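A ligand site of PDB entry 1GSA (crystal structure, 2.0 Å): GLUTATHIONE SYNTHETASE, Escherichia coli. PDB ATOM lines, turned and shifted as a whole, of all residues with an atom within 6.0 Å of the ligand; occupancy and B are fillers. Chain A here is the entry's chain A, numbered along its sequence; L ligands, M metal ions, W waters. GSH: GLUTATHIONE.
O2 of the ligand is in hydrogen-bond range of N of Thr 288 (3.0 Å). An oxygen (O12) of the ligand is in hydrogen-bond range of the side-chain hydroxyl (OG1) of Thr 288 (2.7 Å). N1 of the ligand lies within salt-bridge range of OD1 of Asp 88 (2.8 Å). NH1 of Arg 210 lies within hydrogen-bond range of O2 of the ligand, 2.8 Å away. An oxygen (O11) of the ligand lies within salt-bridge range of the guanidinium group of Arg 86, at 2.9 Å. A nitrogen (N2) of the ligand lies within hydrogen-bond range of the backbone carbonyl oxygen (O) of Ser 286 (3.1 Å). A nitrogen (N1) of the ligand sits at hydrogen-bond distance from the side-chain hydroxyl (OG) of Ser 286, 2.9 Å away. An oxygen (O32) of the ligand is in salt-bridge range of the guanidinium group of Arg 225 (3.0 Å). The backbone NH of Ser 20 sits at hydrogen-bond distance from an oxygen (O11) of the ligand, at 3.0 Å. The backbone NH (N) of Leu 236 sits at hydrogen-bond distance from an oxygen (O32) of the ligand, 3.1 Å away. N of Ala 237 lies within hydrogen-bond range of O31 of the ligand (3.4 Å). N of Ser 21 lies within hydrogen-bond range of O11 of the ligand, 3.4 Å away. A sulfur (SG2) of the ligand lies close to the side-chain hydroxyl (OG1) of Thr 285.
Water W2 lies within hydrogen-bond range of the side-chain hydroxyl (OG) of Ser 21 (2.6 Å), a nitrogen (N1) of the ligand (2.9 Å) and the side-chain carboxylate (OD2) of Asp 19 (3.1 Å).
The side-chain hydroxyl of Thr 288 is in hydrogen-bond range of the side-chain hydroxyl of Ser 20 (2.8 Å). The side-chain carboxylate (OD1) of Asp 88 is in hydrogen-bond range of the side-chain hydroxyl (OG) of Ser 286 (3.1 Å). NH2 of Arg 210 sits close to ND2 of Asn 283 (2.9 Å). The side-chain hydroxyl (OG) of Ser 286 sits at hydrogen-bond distance from the backbone carbonyl oxygen (O) of Arg 86 (3.0 Å). The guanidinium group of Arg 86 sits at hydrogen-bond distance from the side-chain hydroxyl of Ser 21 (3.0 Å). The guanidinium group (NH2) of Arg 86 sits at hydrogen-bond distance from the backbone carbonyl oxygen (O) of Pro 287, at 2.9 Å. N of Ser 21 sits at hydrogen-bond distance from OD1 of Asp 19 (3.0 Å). N of Phe 22 is in hydrogen-bond range of OD1 of Asp 19, 3.0 Å away.
Lys 18 touches the ligand (O to O12, 3.8 Å). CA of Asp 19 touches O12 of the ligand, at 3.4 Å. Pro 89 touches the ligand (CD to SG2, 3.4 Å). Met 165 touches the ligand. CB of Asn 235 touches O31 of the ligand, at 3.9 Å. Pro 287 touches the ligand (CA to O2, 3.5 Å). Hydrophobic or aromatic side chains that line the ligand: Pro 89, Met 165, Leu 236 and Ala 237. 17 residues have an atom within 4 Å of the ligand: Lys 18, Asp 19, Ser 20, Ser 21, Arg 86, Asp 88, Pro 89, Met 165, Arg 210, Arg 225, Asn 235, Leu 236, Ala 237, Thr 285, Ser 286, Pro 287 and Thr 288.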
ATOM      1  N   ASP A   9      -7.935   1.562 -31.684  1.00  0.00           N
ATOM      2  CA  ASP A   9      -7.718   0.251 -32.264  1.00  0.00           C
ATOM      3  C   ASP A   9      -9.092  -0.401 -32.344  1.00  0.00           C
ATOM      4  O   ASP A   9     -10.026   0.044 -31.669  1.00  0.00           O
ATOM      5  CB  ASP A   9      -6.824  -0.582 -31.365  1.00  0.00           C
ATOM      6  CG  ASP A   9      -5.423  -0.057 -31.233  1.00  0.00           C
ATOM      7  OD1 ASP A   9      -4.584  -0.425 -32.050  1.00  0.00           O
ATOM      8  OD2 ASP A   9      -5.168   0.736 -30.325  1.00  0.00           O
ATOM      9  N   LYS A  18     -12.026  -4.086 -19.034  1.00  0.00           N
ATOM     10  CA  LYS A  18     -10.778  -3.455 -18.673  1.00  0.00           C
ATOM     11  C   LYS A  18     -10.547  -2.216 -19.476  1.00  0.00           C
ATOM     12  O   LYS A  18      -9.736  -1.393 -19.056  1.00  0.00           O
ATOM     13  CB  LYS A  18      -9.596  -4.351 -18.976  1.00  0.00           C
ATOM     14  CG  LYS A  18      -9.416  -5.664 -18.220  1.00  0.00           C
ATOM     15  CD  LYS A  18      -9.065  -5.409 -16.735  1.00  0.00           C
ATOM     16  CE  LYS A  18      -7.826  -6.165 -16.156  1.00  0.00           C
ATOM     17  NZ  LYS A  18      -7.432  -5.690 -14.820  1.00  0.00           N
ATOM     18  N   ASP A  19     -11.184  -2.068 -20.617  1.00  0.00           N
ATOM     19  CA  ASP A  19     -10.787  -0.997 -21.508  1.00  0.00           C
ATOM     20  C   ASP A  19     -11.155   0.406 -21.056  1.00  0.00           C
ATOM     21  O   ASP A  19     -12.317   0.710 -20.772  1.00  0.00           O
ATOM     22  CB  ASP A  19     -11.350  -1.282 -22.892  1.00  0.00           C
ATOM     23  CG  ASP A  19     -10.688  -0.450 -23.993  1.00  0.00           C
ATOM     24  OD1 ASP A  19     -11.168   0.650 -24.265  1.00  0.00           O
ATOM     25  OD2 ASP A  19      -9.719  -0.883 -24.611  1.00  0.00           O
ATOM     26  N   SER A  20     -10.192   1.314 -21.006  1.00  0.00           N
ATOM     27  CA  SER A  20     -10.545   2.667 -20.619  1.00  0.00           C
ATOM     28  C   SER A  20     -11.119   3.492 -21.756  1.00  0.00           C
ATOM     29  O   SER A  20     -11.933   4.350 -21.430  1.00  0.00           O
ATOM     30  CB  SER A  20      -9.328   3.377 -20.046  1.00  0.00           C
ATOM     31  OG  SER A  20      -8.886   2.649 -18.899  1.00  0.00           O
ATOM     32  N   SER A  21     -10.792   3.350 -23.062  1.00  0.00           N
ATOM     33  CA  SER A  21     -11.448   4.139 -24.092  1.00  0.00           C
ATOM     34  C   SER A  21     -12.952   3.901 -24.002  1.00  0.00           C
ATOM     35  O   SER A  21     -13.728   4.835 -24.053  1.00  0.00           O
ATOM     36  CB  SER A  21     -10.977   3.738 -25.461  1.00  0.00           C
ATOM     37  OG  SER A  21      -9.573   3.734 -25.521  1.00  0.00           O
ATOM     38  N   PHE A  22     -13.365   2.664 -23.773  1.00  0.00           N
ATOM     39  CA  PHE A  22     -14.747   2.281 -23.704  1.00  0.00           C
ATOM     40  C   PHE A  22     -15.432   2.954 -22.509  1.00  0.00           C
ATOM     41  O   PHE A  22     -16.465   3.582 -22.681  1.00  0.00           O
ATOM     42  CB  PHE A  22     -14.779   0.774 -23.636  1.00  0.00           C
ATOM     43  CG  PHE A  22     -16.205   0.275 -23.774  1.00  0.00           C
ATOM     44  CD1 PHE A  22     -16.804   0.256 -25.044  1.00  0.00           C
ATOM     45  CD2 PHE A  22     -16.909  -0.116 -22.636  1.00  0.00           C
ATOM     46  CE1 PHE A  22     -18.122  -0.165 -25.153  1.00  0.00           C
ATOM     47  CE2 PHE A  22     -18.231  -0.534 -22.754  1.00  0.00           C
ATOM     48  CZ  PHE A  22     -18.840  -0.556 -24.010  1.00  0.00           C
ATOM     49  N   ARG A  86      -6.759   7.752 -28.928  1.00  0.00           N
ATOM     50  CA  ARG A  86      -6.581   6.626 -28.049  1.00  0.00           C
ATOM     51  C   ARG A  86      -5.927   5.441 -28.747  1.00  0.00           C
ATOM     52  O   ARG A  86      -6.144   4.304 -28.326  1.00  0.00           O
ATOM     53  CB  ARG A  86      -7.953   6.267 -27.524  1.00  0.00           C
ATOM     54  CG  ARG A  86      -8.569   7.230 -26.531  1.00  0.00           C
ATOM     55  CD  ARG A  86      -7.806   7.241 -25.201  1.00  0.00           C
ATOM     56  NE  ARG A  86      -7.864   5.971 -24.501  1.00  0.00           N
ATOM     57  CZ  ARG A  86      -7.267   5.767 -23.330  1.00  0.00           C
ATOM     58  NH1 ARG A  86      -6.572   6.711 -22.722  1.00  0.00           N
ATOM     59  NH2 ARG A  86      -7.352   4.589 -22.747  1.00  0.00           N
ATOM     60  N   ASP A  88      -3.177   2.731 -29.511  1.00  0.00           N
ATOM     61  CA  ASP A  88      -2.164   2.119 -28.655  1.00  0.00           C
ATOM     62  C   ASP A  88      -0.807   2.226 -29.249  1.00  0.00           C
ATOM     63  O   ASP A  88      -0.682   2.230 -30.484  1.00  0.00           O
ATOM     64  CB  ASP A  88      -2.379   0.631 -28.405  1.00  0.00           C
ATOM     65  CG  ASP A  88      -3.539   0.355 -27.490  1.00  0.00           C
ATOM     66  OD1 ASP A  88      -3.920   1.229 -26.707  1.00  0.00           O
ATOM     67  OD2 ASP A  88      -4.080  -0.741 -27.581  1.00  0.00           O
ATOM     68  N   PRO A  89       0.245   2.242 -28.417  1.00  0.00           N
ATOM     69  CA  PRO A  89       1.621   2.133 -28.896  1.00  0.00           C
ATOM     70  C   PRO A  89       1.797   0.835 -29.678  1.00  0.00           C
ATOM     71  O   PRO A  89       0.878   0.003 -29.643  1.00  0.00           O
ATOM     72  CB  PRO A  89       2.442   2.237 -27.635  1.00  0.00           C
ATOM     73  CG  PRO A  89       1.592   3.060 -26.755  1.00  0.00           C
ATOM     74  CD  PRO A  89       0.221   2.424 -26.976  1.00  0.00           C
ATOM     75  N   GLU A 124       7.019   8.424 -24.195  1.00  0.00           N
ATOM     76  CA  GLU A 124       6.724   7.862 -22.879  1.00  0.00           C
ATOM     77  C   GLU A 124       7.931   7.495 -22.040  1.00  0.00           C
ATOM     78  O   GLU A 124       7.907   7.587 -20.813  1.00  0.00           O
ATOM     79  CB  GLU A 124       5.814   6.653 -23.060  1.00  0.00           C
ATOM     80  CG  GLU A 124       4.521   7.105 -23.777  1.00  0.00           C
ATOM     81  CD  GLU A 124       3.385   6.107 -23.935  1.00  0.00           C
ATOM     82  OE1 GLU A 124       3.604   4.905 -24.042  1.00  0.00           O
ATOM     83  OE2 GLU A 124       2.243   6.528 -23.953  1.00  0.00           O
ATOM     84  N   MET A 165       5.195  -0.550 -24.685  1.00  0.00           N
ATOM     85  CA  MET A 165       4.515  -0.344 -23.422  1.00  0.00           C
ATOM     86  C   MET A 165       4.139  -1.746 -22.946  1.00  0.00           C
ATOM     87  O   MET A 165       4.453  -2.730 -23.628  1.00  0.00           O
ATOM     88  CB  MET A 165       3.265   0.528 -23.609  1.00  0.00           C
ATOM     89  CG  MET A 165       1.957  -0.068 -24.138  1.00  0.00           C
ATOM     90  SD  MET A 165       2.141  -0.997 -25.694  1.00  0.00           S
ATOM     91  CE  MET A 165       0.560  -1.792 -25.556  1.00  0.00           C
ATOM     92  N   GLY A 166       3.525  -1.907 -21.761  1.00  0.00           N
ATOM     93  CA  GLY A 166       3.079  -3.223 -21.312  1.00  0.00           C
ATOM     94  C   GLY A 166       4.161  -4.253 -20.947  1.00  0.00           C
ATOM     95  O   GLY A 166       3.862  -5.441 -20.776  1.00  0.00           O
ATOM     96  N   ARG A 210       0.199   3.041 -11.155  1.00  0.00           N
ATOM     97  CA  ARG A 210      -0.276   3.883 -12.223  1.00  0.00           C
ATOM     98  C   ARG A 210      -1.005   5.016 -11.525  1.00  0.00           C
ATOM     99  O   ARG A 210      -2.004   4.771 -10.834  1.00  0.00           O
ATOM    100  CB  ARG A 210      -1.223   3.095 -13.114  1.00  0.00           C
ATOM    101  CG  ARG A 210      -2.110   3.947 -14.054  1.00  0.00           C
ATOM    102  CD  ARG A 210      -1.375   5.013 -14.901  1.00  0.00           C
ATOM    103  NE  ARG A 210      -0.278   4.449 -15.648  1.00  0.00           N
ATOM    104  CZ  ARG A 210      -0.442   3.596 -16.661  1.00  0.00           C
ATOM    105  NH1 ARG A 210      -1.616   3.186 -17.105  1.00  0.00           N
ATOM    106  NH2 ARG A 210       0.602   3.045 -17.220  1.00  0.00           N
ATOM    107  N   LEU A 223      -3.470   2.641  -8.876  1.00  0.00           N
ATOM    108  CA  LEU A 223      -3.558   1.209  -8.986  1.00  0.00           C
ATOM    109  C   LEU A 223      -2.120   0.746  -8.854  1.00  0.00           C
ATOM    110  O   LEU A 223      -1.321   1.178  -9.682  1.00  0.00           O
ATOM    111  CB  LEU A 223      -4.058   0.725 -10.364  1.00  0.00           C
ATOM    112  CG  LEU A 223      -4.214  -0.789 -10.585  1.00  0.00           C
ATOM    113  CD1 LEU A 223      -5.521  -1.180  -9.961  1.00  0.00           C
ATOM    114  CD2 LEU A 223      -4.329  -1.187 -12.020  1.00  0.00           C
ATOM    115  N   ARG A 225       0.594  -2.101  -9.448  1.00  0.00           N
ATOM    116  CA  ARG A 225       0.632  -3.326 -10.236  1.00  0.00           C
ATOM    117  C   ARG A 225       1.778  -4.177  -9.708  1.00  0.00           C
ATOM    118  O   ARG A 225       2.963  -3.801  -9.742  1.00  0.00           O
ATOM    119  CB  ARG A 225       0.843  -2.981 -11.730  1.00  0.00           C
ATOM    120  CG  ARG A 225      -0.319  -2.254 -12.389  1.00  0.00           C
ATOM    121  CD  ARG A 225       0.060  -0.811 -12.688  1.00  0.00           C
ATOM    122  NE  ARG A 225       0.244  -0.637 -14.113  1.00  0.00           N
ATOM    123  CZ  ARG A 225       1.186   0.103 -14.657  1.00  0.00           C
ATOM    124  NH1 ARG A 225       2.105   0.788 -13.975  1.00  0.00           N
ATOM    125  NH2 ARG A 225       1.179   0.139 -15.968  1.00  0.00           N
ATOM    126  N   GLY A 234       5.619  -5.686 -13.744  1.00  0.00           N
ATOM    127  CA  GLY A 234       4.447  -5.332 -12.956  1.00  0.00           C
ATOM    128  C   GLY A 234       3.211  -5.111 -13.817  1.00  0.00           C
ATOM    129  O   GLY A 234       2.097  -5.296 -13.366  1.00  0.00           O
ATOM    130  N   ASN A 235       3.379  -4.673 -15.070  1.00  0.00           N
ATOM    131  CA  ASN A 235       2.312  -4.450 -16.045  1.00  0.00           C
ATOM    132  C   ASN A 235       1.151  -5.407 -16.017  1.00  0.00           C
ATOM    133  O   ASN A 235       1.377  -6.614 -16.084  1.00  0.00           O
ATOM    134  CB  ASN A 235       2.820  -4.517 -17.471  1.00  0.00           C
ATOM    135  CG  ASN A 235       3.943  -3.549 -17.691  1.00  0.00           C
ATOM    136  OD1 ASN A 235       5.103  -3.869 -17.451  1.00  0.00           O
ATOM    137  ND2 ASN A 235       3.653  -2.346 -18.166  1.00  0.00           N
ATOM    138  N   LEU A 236      -0.094  -4.934 -16.006  1.00  0.00           N
ATOM    139  CA  LEU A 236      -1.251  -5.832 -16.116  1.00  0.00           C
ATOM    140  C   LEU A 236      -1.142  -6.659 -17.395  1.00  0.00           C
ATOM    141  O   LEU A 236      -1.483  -7.846 -17.408  1.00  0.00           O
ATOM    142  CB  LEU A 236      -2.576  -5.075 -16.178  1.00  0.00           C
ATOM    143  CG  LEU A 236      -2.977  -4.208 -15.004  1.00  0.00           C
ATOM    144  CD1 LEU A 236      -4.334  -3.585 -15.327  1.00  0.00           C
ATOM    145  CD2 LEU A 236      -3.014  -5.032 -13.727  1.00  0.00           C
ATOM    146  N   ALA A 237      -0.595  -6.007 -18.443  1.00  0.00           N
ATOM    147  CA  ALA A 237      -0.336  -6.631 -19.736  1.00  0.00           C
ATOM    148  C   ALA A 237       0.574  -7.837 -19.671  1.00  0.00           C
ATOM    149  O   ALA A 237       0.468  -8.779 -20.455  1.00  0.00           O
ATOM    150  CB  ALA A 237       0.282  -5.593 -20.660  1.00  0.00           C
ATOM    151  N   ALA A 238       1.506  -7.874 -18.713  1.00  0.00           N
ATOM    152  CA  ALA A 238       2.406  -9.005 -18.545  1.00  0.00           C
ATOM    153  C   ALA A 238       1.967  -9.724 -17.280  1.00  0.00           C
ATOM    154  O   ALA A 238       2.812 -10.103 -16.470  1.00  0.00           O
ATOM    155  CB  ALA A 238       3.845  -8.504 -18.389  1.00  0.00           C
ATOM    156  N   ASN A 283       2.911   7.867 -19.600  1.00  0.00           N
ATOM    157  CA  ASN A 283       2.078   7.425 -20.693  1.00  0.00           C
ATOM    158  C   ASN A 283       1.091   8.482 -21.084  1.00  0.00           C
ATOM    159  O   ASN A 283       0.193   8.878 -20.348  1.00  0.00           O
ATOM    160  CB  ASN A 283       1.330   6.127 -20.351  1.00  0.00           C
ATOM    161  CG  ASN A 283       2.397   5.078 -20.074  1.00  0.00           C
ATOM    162  OD1 ASN A 283       3.271   4.818 -20.894  1.00  0.00           O
ATOM    163  ND2 ASN A 283       2.522   4.483 -18.907  1.00  0.00           N
ATOM    164  N   THR A 285      -0.185   8.317 -24.627  1.00  0.00           N
ATOM    165  CA  THR A 285      -0.978   7.885 -25.775  1.00  0.00           C
ATOM    166  C   THR A 285      -2.322   7.237 -25.413  1.00  0.00           C
ATOM    167  O   THR A 285      -3.362   7.816 -25.752  1.00  0.00           O
ATOM    168  CB  THR A 285      -0.122   6.926 -26.642  1.00  0.00           C
ATOM    169  OG1 THR A 285       0.346   5.916 -25.766  1.00  0.00           O
ATOM    170  CG2 THR A 285       1.092   7.575 -27.267  1.00  0.00           C
ATOM    171  N   SER A 286      -2.354   6.083 -24.743  1.00  0.00           N
ATOM    172  CA  SER A 286      -3.574   5.406 -24.368  1.00  0.00           C
ATOM    173  C   SER A 286      -3.521   4.789 -22.961  1.00  0.00           C
ATOM    174  O   SER A 286      -3.738   3.574 -22.795  1.00  0.00           O
ATOM    175  CB  SER A 286      -3.826   4.362 -25.461  1.00  0.00           C
ATOM    176  OG  SER A 286      -5.142   3.807 -25.567  1.00  0.00           O
ATOM    177  N   PRO A 287      -3.195   5.521 -21.876  1.00  0.00           N
ATOM    178  CA  PRO A 287      -3.149   4.994 -20.528  1.00  0.00           C
ATOM    179  C   PRO A 287      -4.491   4.450 -20.092  1.00  0.00           C
ATOM    180  O   PRO A 287      -5.559   4.927 -20.451  1.00  0.00           O
ATOM    181  CB  PRO A 287      -2.652   6.166 -19.693  1.00  0.00           C
ATOM    182  CG  PRO A 287      -3.104   7.391 -20.412  1.00  0.00           C
ATOM    183  CD  PRO A 287      -2.861   6.948 -21.855  1.00  0.00           C
ATOM    184  N   THR A 288      -4.395   3.338 -19.400  1.00  0.00           N
ATOM    185  CA  THR A 288      -5.564   2.691 -18.879  1.00  0.00           C
ATOM    186  C   THR A 288      -5.546   2.632 -17.348  1.00  0.00           C
ATOM    187  O   THR A 288      -4.953   3.510 -16.734  1.00  0.00           O
ATOM    188  CB  THR A 288      -5.548   1.360 -19.647  1.00  0.00           C
ATOM    189  OG1 THR A 288      -6.874   0.848 -19.526  1.00  0.00           O
ATOM    190  CG2 THR A 288      -4.512   0.370 -19.198  1.00  0.00           C
ATOM    191  N   CYS A 289      -6.209   1.661 -16.719  1.00  0.00           N
ATOM    192  CA  CYS A 289      -6.422   1.459 -15.291  1.00  0.00           C
ATOM    193  C   CYS A 289      -7.616   2.213 -14.728  1.00  0.00           C
ATOM    194  O   CYS A 289      -7.923   2.048 -13.544  1.00  0.00           O
ATOM    195  CB  CYS A 289      -5.177   1.823 -14.479  1.00  0.00           C
ATOM    196  SG  CYS A 289      -3.875   0.680 -14.998  1.00  0.00           S
HETATM  197  N1  GSH L   1      -6.127   1.116 -25.017  1.00  0.00           N
HETATM  198  CA1 GSH L   1      -6.135   0.360 -23.785  1.00  0.00           C
HETATM  199  C1  GSH L   1      -7.220   0.670 -22.776  1.00  0.00           C
HETATM  200  O11 GSH L   1      -7.791   1.767 -22.818  1.00  0.00           O
HETATM  201  O12 GSH L   1      -7.466  -0.185 -21.919  1.00  0.00           O
HETATM  202  CB1 GSH L   1      -4.811   0.529 -23.092  1.00  0.00           C
HETATM  203  CG1 GSH L   1      -3.687  -0.204 -23.767  1.00  0.00           C
HETATM  204  CD1 GSH L   1      -2.418  -0.155 -22.936  1.00  0.00           C
HETATM  205  OE1 GSH L   1      -1.827  -1.209 -22.623  1.00  0.00           O
HETATM  206  N2  GSH L   1      -1.997   1.050 -22.527  1.00  0.00           N
HETATM  207  CA2 GSH L   1      -0.809   1.169 -21.712  1.00  0.00           C
HETATM  208  C2  GSH L   1      -1.240   1.009 -20.261  1.00  0.00           C
HETATM  209  O2  GSH L   1      -1.794   1.921 -19.647  1.00  0.00           O
HETATM  210  CB2 GSH L   1      -0.181   2.533 -21.881  1.00  0.00           C
HETATM  211  SG2 GSH L   1      -0.197   2.998 -23.611  1.00  0.00           S
HETATM  212  N3  GSH L   1      -0.939  -0.155 -19.691  1.00  0.00           N
HETATM  213  CA3 GSH L   1      -1.211  -0.413 -18.282  1.00  0.00           C
HETATM  214  C3  GSH L   1      -0.742  -1.793 -17.835  1.00  0.00           C
HETATM  215  O31 GSH L   1      -0.370  -2.659 -18.646  1.00  0.00           O
HETATM  216  O32 GSH L   1      -0.769  -2.006 -16.621  1.00  0.00           O
HETATM  217 MG    MG M   1       4.071   2.719 -20.671  1.00  0.00          MG
HETATM  218  O   HOH W   1      -2.530  -2.978 -20.453  1.00  0.00           O
HETATM  219  O   HOH W   2      -8.659   1.466 -26.293  1.00  0.00           O
